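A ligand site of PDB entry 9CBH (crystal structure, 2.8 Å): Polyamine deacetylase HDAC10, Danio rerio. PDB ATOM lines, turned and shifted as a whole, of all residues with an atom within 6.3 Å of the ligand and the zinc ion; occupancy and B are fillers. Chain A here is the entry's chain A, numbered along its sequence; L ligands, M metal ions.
CD1 of Ile 27 touches C4 of the ligand, at 3.96 Å. Ala 94 touches the ligand. Gly 145 touches the ligand (O to C7, 3.3 Å). Phe 146 touches the ligand (CE2 to C5, 3.4 Å). Trp 205 touches the ligand. Hydrophobic or aromatic side chains that line the ligand: Ile 27, Ala 94, His 136, His 137, Phe 146, His 176, Trp 205 and Tyr 307.
A ring nitrogen (NE2) of His 136 sits close to a sulfur (S1) of the ligand (3.1 Å). The side-chain hydroxyl (OH) of Tyr 307 sits close to an oxygen (O1) of the ligand. N1 of the ligand lies within hydrogen-bond range of O of Glu 24 (3.1 Å). A ring nitrogen (ND1) of His 137 sits close to a sulfur (S1) of the ligand (3.6 Å). A nitrogen (N1) of the ligand lies within salt-bridge range of the side-chain carboxylate (OE2) of Glu 274 (3.96 Å).
The side-chain carboxylate (OD1) of Asp 267 lies within hydrogen-bond range of the backbone NH (N) of Val 175 (2.8 Å). The backbone NH (N) of His 136 lies close to the side-chain carboxylate (OE1) of Glu 304, 3.1 Å away. The backbone carbonyl oxygen (O) of Gly 145 sits at hydrogen-bond distance from the side-chain sulfur (SG) of Cys 147. The side-chain sulfur of Cys 147 is in hydrogen-bond range of the backbone NH of His 137, 3.4 Å away. The backbone NH (N) of Gly 145 sits at hydrogen-bond distance from the backbone carbonyl oxygen (O) of Asn 93. O of Ala 94 is in hydrogen-bond range of N of Phe 146 (2.9 Å). The backbone NH (N) of Gly 145 sits close to the backbone carbonyl oxygen (O) of Ala 94. OD2 of Asp 174 sits close to N of Gly 305 (2.9 Å).
OD2 of Asp 267 is bound to the zinc ion (2.0 Å). OD1 of Asp 174 is bound to the zinc ion. ND1 of His 176 is bound to the zinc ion (2.3 Å). S1 of the ligand is bound to the zinc ion (2.3 Å). OD2 of Asp 174 binds the zinc ion (2.5 Å). The zinc ion has five donor atoms within binding distance. Slightly farther from the zinc ion lies an oxygen (O1) of the ligand (2.8 Å).
Within 4 Å of the zinc ion: Asp 174, His 176 and Asp 267.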
ATOM      1  N   PRO A  23      -1.632  -3.967  17.341  1.00  0.00           N
ATOM      2  CA  PRO A  23      -2.076  -2.670  17.900  1.00  0.00           C
ATOM      3  C   PRO A  23      -1.440  -2.343  19.235  1.00  0.00           C
ATOM      4  O   PRO A  23      -1.293  -1.159  19.564  1.00  0.00           O
ATOM      5  CB  PRO A  23      -3.589  -2.842  18.030  1.00  0.00           C
ATOM      6  CG  PRO A  23      -3.932  -3.932  17.061  1.00  0.00           C
ATOM      7  CD  PRO A  23      -2.763  -4.864  17.079  1.00  0.00           C
ATOM      8  N   GLU A  24      -1.027  -3.350  20.003  1.00  0.00           N
ATOM      9  CA  GLU A  24      -0.378  -3.091  21.284  1.00  0.00           C
ATOM     10  C   GLU A  24       0.919  -2.320  21.104  1.00  0.00           C
ATOM     11  O   GLU A  24       1.329  -1.572  21.997  1.00  0.00           O
ATOM     12  CB  GLU A  24      -0.126  -4.403  22.030  1.00  0.00           C
ATOM     13  N   CYS A  25       1.573  -2.468  19.954  1.00  0.00           N
ATOM     14  CA  CYS A  25       2.867  -1.848  19.711  1.00  0.00           C
ATOM     15  C   CYS A  25       2.856  -0.845  18.564  1.00  0.00           C
ATOM     16  O   CYS A  25       3.912  -0.294  18.232  1.00  0.00           O
ATOM     17  CB  CYS A  25       3.921  -2.920  19.433  1.00  0.00           C
ATOM     18  SG  CYS A  25       4.099  -4.164  20.733  1.00  0.00           S
ATOM     19  N   ILE A  27       2.128   2.119  18.305  1.00  0.00           N
ATOM     20  CA  ILE A  27       2.554   3.480  18.634  1.00  0.00           C
ATOM     21  C   ILE A  27       4.059   3.617  18.525  1.00  0.00           C
ATOM     22  O   ILE A  27       4.565   4.677  18.140  1.00  0.00           O
ATOM     23  CB  ILE A  27       2.062   3.867  20.035  1.00  0.00           C
ATOM     24  CG1 ILE A  27       2.456   2.799  21.045  1.00  0.00           C
ATOM     25  CG2 ILE A  27       0.563   4.084  20.033  1.00  0.00           C
ATOM     26  CD1 ILE A  27       2.188   3.179  22.462  1.00  0.00           C
ATOM     27  N   ASN A  93       5.673  -9.582  26.831  1.00  0.00           N
ATOM     28  CA  ASN A  93       4.477  -8.760  26.983  1.00  0.00           C
ATOM     29  C   ASN A  93       4.693  -7.387  26.365  1.00  0.00           C
ATOM     30  O   ASN A  93       5.591  -6.641  26.791  1.00  0.00           O
ATOM     31  CB  ASN A  93       4.093  -8.636  28.453  1.00  0.00           C
ATOM     32  CG  ASN A  93       2.706  -8.068  28.654  1.00  0.00           C
ATOM     33  OD1 ASN A  93       2.545  -6.900  29.014  1.00  0.00           O
ATOM     34  ND2 ASN A  93       1.689  -8.882  28.404  1.00  0.00           N
ATOM     35  N   ALA A  94       3.867  -7.048  25.367  1.00  0.00           N
ATOM     36  CA  ALA A  94       3.817  -5.717  24.775  1.00  0.00           C
ATOM     37  C   ALA A  94       5.148  -5.337  24.118  1.00  0.00           C
ATOM     38  O   ALA A  94       5.670  -4.237  24.299  1.00  0.00           O
ATOM     39  CB  ALA A  94       3.404  -4.659  25.811  1.00  0.00           C
ATOM     40  N   PRO A 134      13.300   1.813  24.277  1.00  0.00           N
ATOM     41  CA  PRO A 134      13.421   2.249  25.678  1.00  0.00           C
ATOM     42  C   PRO A 134      13.916   1.144  26.599  1.00  0.00           C
ATOM     43  O   PRO A 134      14.356   0.087  26.136  1.00  0.00           O
ATOM     44  CB  PRO A 134      11.984   2.677  26.031  1.00  0.00           C
ATOM     45  CG  PRO A 134      11.331   2.955  24.716  1.00  0.00           C
ATOM     46  CD  PRO A 134      11.931   1.971  23.762  1.00  0.00           C
ATOM     47  N   HIS A 136      12.993   1.107  30.699  1.00  0.00           N
ATOM     48  CA  HIS A 136      12.541   0.977  32.092  1.00  0.00           C
ATOM     49  C   HIS A 136      11.616  -0.220  32.319  1.00  0.00           C
ATOM     50  O   HIS A 136      11.519  -0.705  33.451  1.00  0.00           O
ATOM     51  CB  HIS A 136      11.877   2.266  32.574  1.00  0.00           C
ATOM     52  CG  HIS A 136      10.603   2.613  31.854  1.00  0.00           C
ATOM     53  ND1 HIS A 136       9.755   3.603  32.296  1.00  0.00           N
ATOM     54  CD2 HIS A 136      10.046   2.115  30.720  1.00  0.00           C
ATOM     55  CE1 HIS A 136       8.727   3.705  31.469  1.00  0.00           C
ATOM     56  NE2 HIS A 136       8.880   2.815  30.510  1.00  0.00           N
ATOM     57  N   HIS A 137      10.940  -0.712  31.281  1.00  0.00           N
ATOM     58  CA  HIS A 137      10.111  -1.909  31.436  1.00  0.00           C
ATOM     59  C   HIS A 137      10.908  -3.191  31.287  1.00  0.00           C
ATOM     60  O   HIS A 137      10.429  -4.250  31.703  1.00  0.00           O
ATOM     61  CB  HIS A 137       8.970  -1.904  30.418  1.00  0.00           C
ATOM     62  CG  HIS A 137       7.919  -0.890  30.691  1.00  0.00           C
ATOM     63  ND1 HIS A 137       7.643   0.159  29.830  1.00  0.00           N
ATOM     64  CD2 HIS A 137       7.072  -0.741  31.741  1.00  0.00           C
ATOM     65  CE1 HIS A 137       6.675   0.893  30.334  1.00  0.00           C
ATOM     66  NE2 HIS A 137       6.307   0.375  31.490  1.00  0.00           N
ATOM     67  N   ASN A 144       9.918  -6.331  27.660  1.00  0.00           N
ATOM     68  CA  ASN A 144       8.627  -5.908  28.161  1.00  0.00           C
ATOM     69  C   ASN A 144       8.372  -4.466  27.754  1.00  0.00           C
ATOM     70  O   ASN A 144       9.286  -3.643  27.787  1.00  0.00           O
ATOM     71  CB  ASN A 144       8.546  -6.056  29.686  1.00  0.00           C
ATOM     72  CG  ASN A 144       7.189  -5.691  30.243  1.00  0.00           C
ATOM     73  OD1 ASN A 144       6.995  -4.588  30.735  1.00  0.00           O
ATOM     74  ND2 ASN A 144       6.249  -6.616  30.156  1.00  0.00           N
ATOM     75  N   GLY A 145       7.129  -4.169  27.379  1.00  0.00           N
ATOM     76  CA  GLY A 145       6.684  -2.821  27.073  1.00  0.00           C
ATOM     77  C   GLY A 145       7.638  -2.030  26.207  1.00  0.00           C
ATOM     78  O   GLY A 145       8.136  -0.983  26.628  1.00  0.00           O
ATOM     79  N   PHE A 146       7.919  -2.543  25.008  1.00  0.00           N
ATOM     80  CA  PHE A 146       8.781  -1.919  23.996  1.00  0.00           C
ATOM     81  C   PHE A 146      10.233  -1.835  24.436  1.00  0.00           C
ATOM     82  O   PHE A 146      11.021  -1.107  23.815  1.00  0.00           O
ATOM     83  CB  PHE A 146       8.301  -0.505  23.619  1.00  0.00           C
ATOM     84  CG  PHE A 146       6.825  -0.403  23.336  1.00  0.00           C
ATOM     85  CD1 PHE A 146       6.094  -1.499  22.890  1.00  0.00           C
ATOM     86  CD2 PHE A 146       6.162   0.806  23.496  1.00  0.00           C
ATOM     87  CE1 PHE A 146       4.745  -1.396  22.642  1.00  0.00           C
ATOM     88  CE2 PHE A 146       4.808   0.917  23.245  1.00  0.00           C
ATOM     89  CZ  PHE A 146       4.103  -0.185  22.808  1.00  0.00           C
ATOM     90  N   CYS A 147      10.639  -2.565  25.477  1.00  0.00           N
ATOM     91  CA  CYS A 147      11.995  -2.524  26.003  1.00  0.00           C
ATOM     92  C   CYS A 147      12.633  -3.887  25.858  1.00  0.00           C
ATOM     93  O   CYS A 147      12.046  -4.900  26.243  1.00  0.00           O
ATOM     94  CB  CYS A 147      12.015  -2.094  27.464  1.00  0.00           C
ATOM     95  SG  CYS A 147      11.004  -0.647  27.833  1.00  0.00           S
ATOM     96  N   ASP A 174       8.161   8.967  32.849  1.00  0.00           N
ATOM     97  CA  ASP A 174       7.341   8.304  31.848  1.00  0.00           C
ATOM     98  C   ASP A 174       6.002   7.919  32.460  1.00  0.00           C
ATOM     99  O   ASP A 174       5.898   7.602  33.651  1.00  0.00           O
ATOM    100  CB  ASP A 174       8.071   7.066  31.322  1.00  0.00           C
ATOM    101  CG  ASP A 174       7.310   6.361  30.217  1.00  0.00           C
ATOM    102  OD1 ASP A 174       6.346   5.630  30.521  1.00  0.00           O
ATOM    103  OD2 ASP A 174       7.676   6.524  29.036  1.00  0.00           O
ATOM    104  N   VAL A 175       4.945   7.985  31.648  1.00  0.00           N
ATOM    105  CA  VAL A 175       3.596   7.761  32.180  1.00  0.00           C
ATOM    106  C   VAL A 175       3.357   6.314  32.584  1.00  0.00           C
ATOM    107  O   VAL A 175       2.418   6.034  33.328  1.00  0.00           O
ATOM    108  CB  VAL A 175       2.522   8.215  31.171  1.00  0.00           C
ATOM    109  CG1 VAL A 175       2.212   7.103  30.183  1.00  0.00           C
ATOM    110  CG2 VAL A 175       1.260   8.653  31.915  1.00  0.00           C
ATOM    111  N   HIS A 176       4.191   5.393  32.121  1.00  0.00           N
ATOM    112  CA  HIS A 176       4.127   4.008  32.549  1.00  0.00           C
ATOM    113  C   HIS A 176       5.107   3.750  33.680  1.00  0.00           C
ATOM    114  O   HIS A 176       6.071   4.496  33.885  1.00  0.00           O
ATOM    115  CB  HIS A 176       4.421   3.057  31.378  1.00  0.00           C
ATOM    116  CG  HIS A 176       3.494   3.231  30.220  1.00  0.00           C
ATOM    117  ND1 HIS A 176       3.666   4.207  29.267  1.00  0.00           N
ATOM    118  CD2 HIS A 176       2.371   2.565  29.868  1.00  0.00           C
ATOM    119  CE1 HIS A 176       2.699   4.136  28.380  1.00  0.00           C
ATOM    120  NE2 HIS A 176       1.893   3.137  28.718  1.00  0.00           N
ATOM    121  N   HIS A 177       4.857   2.668  34.422  1.00  0.00           N
ATOM    122  CA  HIS A 177       5.577   2.382  35.655  1.00  0.00           C
ATOM    123  C   HIS A 177       7.081   2.266  35.417  1.00  0.00           C
ATOM    124  O   HIS A 177       7.819   3.237  35.620  1.00  0.00           O
ATOM    125  CB  HIS A 177       5.049   1.095  36.295  1.00  0.00           C
ATOM    126  CG  HIS A 177       5.673   0.780  37.623  1.00  0.00           C
ATOM    127  ND1 HIS A 177       5.676  -0.490  38.151  1.00  0.00           N
ATOM    128  CD2 HIS A 177       6.312   1.556  38.520  1.00  0.00           C
ATOM    129  CE1 HIS A 177       6.292  -0.484  39.324  1.00  0.00           C
ATOM    130  NE2 HIS A 177       6.691   0.752  39.567  1.00  0.00           N
ATOM    131  N   PHE A 204      -4.514  -0.159  34.542  1.00  0.00           N
ATOM    132  CA  PHE A 204      -3.719   0.284  33.415  1.00  0.00           C
ATOM    133  C   PHE A 204      -2.408  -0.506  33.343  1.00  0.00           C
ATOM    134  O   PHE A 204      -1.840  -0.882  34.370  1.00  0.00           O
ATOM    135  CB  PHE A 204      -3.407   1.786  33.511  1.00  0.00           C
ATOM    136  CG  PHE A 204      -2.817   2.349  32.260  1.00  0.00           C
ATOM    137  CD1 PHE A 204      -3.588   2.487  31.116  1.00  0.00           C
ATOM    138  CD2 PHE A 204      -1.493   2.759  32.225  1.00  0.00           C
ATOM    139  CE1 PHE A 204      -3.049   3.010  29.957  1.00  0.00           C
ATOM    140  CE2 PHE A 204      -0.946   3.288  31.068  1.00  0.00           C
ATOM    141  CZ  PHE A 204      -1.723   3.413  29.934  1.00  0.00           C
ATOM    142  N   TRP A 205      -1.960  -0.738  32.116  1.00  0.00           N
ATOM    143  CA  TRP A 205      -0.750  -1.513  31.891  1.00  0.00           C
ATOM    144  C   TRP A 205       0.422  -0.872  32.635  1.00  0.00           C
ATOM    145  O   TRP A 205       0.523   0.359  32.679  1.00  0.00           O
ATOM    146  CB  TRP A 205      -0.460  -1.615  30.396  1.00  0.00           C
ATOM    147  CG  TRP A 205       0.575  -2.625  30.043  1.00  0.00           C
ATOM    148  CD1 TRP A 205       0.358  -3.925  29.667  1.00  0.00           C
ATOM    149  CD2 TRP A 205       1.991  -2.439  30.037  1.00  0.00           C
ATOM    150  NE1 TRP A 205       1.557  -4.552  29.437  1.00  0.00           N
ATOM    151  CE2 TRP A 205       2.583  -3.668  29.663  1.00  0.00           C
ATOM    152  CE3 TRP A 205       2.828  -1.360  30.331  1.00  0.00           C
ATOM    153  CZ2 TRP A 205       3.954  -3.834  29.563  1.00  0.00           C
ATOM    154  CZ3 TRP A 205       4.192  -1.531  30.228  1.00  0.00           C
ATOM    155  CH2 TRP A 205       4.741  -2.751  29.849  1.00  0.00           C
ATOM    156  N   GLY A 265      10.616   9.556  29.573  1.00  0.00           N
ATOM    157  CA  GLY A 265       9.522   9.216  28.673  1.00  0.00           C
ATOM    158  C   GLY A 265       8.533  10.369  28.637  1.00  0.00           C
ATOM    159  O   GLY A 265       8.196  10.945  29.674  1.00  0.00           O
ATOM    160  N   ASP A 267       5.394  10.261  27.202  1.00  0.00           N
ATOM    161  CA  ASP A 267       3.979   9.929  27.114  1.00  0.00           C
ATOM    162  C   ASP A 267       3.188  10.514  28.277  1.00  0.00           C
ATOM    163  O   ASP A 267       1.958  10.424  28.277  1.00  0.00           O
ATOM    164  CB  ASP A 267       3.806   8.409  27.047  1.00  0.00           C
ATOM    165  CG  ASP A 267       4.754   7.672  27.949  1.00  0.00           C
ATOM    166  OD1 ASP A 267       5.326   8.304  28.854  1.00  0.00           O
ATOM    167  OD2 ASP A 267       4.930   6.451  27.747  1.00  0.00           O
ATOM    168  N   GLU A 274      -1.322   7.237  25.103  1.00  0.00           N
ATOM    169  CA  GLU A 274      -1.203   6.268  26.190  1.00  0.00           C
ATOM    170  C   GLU A 274      -1.416   6.903  27.552  1.00  0.00           C
ATOM    171  O   GLU A 274      -2.199   6.399  28.359  1.00  0.00           O
ATOM    172  CB  GLU A 274       0.172   5.593  26.142  1.00  0.00           C
ATOM    173  CG  GLU A 274       0.317   4.574  25.042  1.00  0.00           C
ATOM    174  CD  GLU A 274      -0.291   3.241  25.391  1.00  0.00           C
ATOM    175  OE1 GLU A 274      -0.348   2.920  26.598  1.00  0.00           O
ATOM    176  OE2 GLU A 274      -0.713   2.502  24.473  1.00  0.00           O
ATOM    177  N   GLU A 304      12.652   7.535  26.974  1.00  0.00           N
ATOM    178  CA  GLU A 304      11.857   6.323  27.131  1.00  0.00           C
ATOM    179  C   GLU A 304      10.662   6.377  26.185  1.00  0.00           C
ATOM    180  O   GLU A 304      10.822   6.253  24.966  1.00  0.00           O
ATOM    181  CB  GLU A 304      11.387   6.162  28.573  1.00  0.00           C
ATOM    182  CG  GLU A 304      12.516   5.906  29.575  1.00  0.00           C
ATOM    183  CD  GLU A 304      12.881   4.431  29.683  1.00  0.00           C
ATOM    184  OE1 GLU A 304      12.152   3.596  29.100  1.00  0.00           O
ATOM    185  OE2 GLU A 304      13.878   4.111  30.356  1.00  0.00           O
ATOM    186  N   GLY A 305       9.461   6.569  26.737  1.00  0.00           N
ATOM    187  CA  GLY A 305       8.256   6.661  25.944  1.00  0.00           C
ATOM    188  C   GLY A 305       8.011   8.065  25.427  1.00  0.00           C
ATOM    189  O   GLY A 305       8.862   8.960  25.506  1.00  0.00           O
ATOM    190  N   GLY A 306       6.808   8.265  24.882  1.00  0.00           N
ATOM    191  CA  GLY A 306       6.458   9.505  24.214  1.00  0.00           C
ATOM    192  C   GLY A 306       6.066   9.245  22.779  1.00  0.00           C
ATOM    193  O   GLY A 306       6.933   9.078  21.917  1.00  0.00           O
ATOM    194  N   TYR A 307       4.762   9.200  22.504  1.00  0.00           N
ATOM    195  CA  TYR A 307       4.275   8.658  21.239  1.00  0.00           C
ATOM    196  C   TYR A 307       3.376   9.601  20.454  1.00  0.00           C
ATOM    197  O   TYR A 307       2.995   9.246  19.328  1.00  0.00           O
ATOM    198  CB  TYR A 307       3.550   7.336  21.493  1.00  0.00           C
ATOM    199  CG  TYR A 307       4.435   6.374  22.242  1.00  0.00           C
ATOM    200  CD1 TYR A 307       5.362   5.591  21.568  1.00  0.00           C
ATOM    201  CD2 TYR A 307       4.387   6.277  23.626  1.00  0.00           C
ATOM    202  CE1 TYR A 307       6.193   4.722  22.248  1.00  0.00           C
ATOM    203  CE2 TYR A 307       5.209   5.416  24.313  1.00  0.00           C
ATOM    204  CZ  TYR A 307       6.114   4.638  23.620  1.00  0.00           C
ATOM    205  OH  TYR A 307       6.940   3.776  24.298  1.00  0.00           O
HETATM  206  C1  LIG L   1       0.899  -1.807  25.893  1.00  0.00           C
HETATM  207  C2  LIG L   1       1.990  -0.757  26.108  1.00  0.00           C
HETATM  208  C3  LIG L   1       1.734   0.577  25.826  1.00  0.00           C
HETATM  209  C4  LIG L   1       2.711   1.530  26.020  1.00  0.00           C
HETATM  210  C5  LIG L   1       3.957   1.161  26.508  1.00  0.00           C
HETATM  211  C6  LIG L   1       5.044   2.220  26.721  1.00  0.00           C
HETATM  212  C7  LIG L   1       6.446   1.800  27.131  1.00  0.00           C
HETATM  213  C8  LIG L   1       4.214  -0.173  26.790  1.00  0.00           C
HETATM  214  C9  LIG L   1       3.233  -1.126  26.606  1.00  0.00           C
HETATM  215  N1  LIG L   1       0.000  -1.372  24.841  1.00  0.00           N
HETATM  216  O1  LIG L   1       4.799   3.370  26.565  1.00  0.00           O
HETATM  217  S1  LIG L   1       7.236   3.209  27.965  1.00  0.00           S
HETATM  218 ZN    ZN M   1       5.771   4.912  28.654  1.00  0.00          ZN
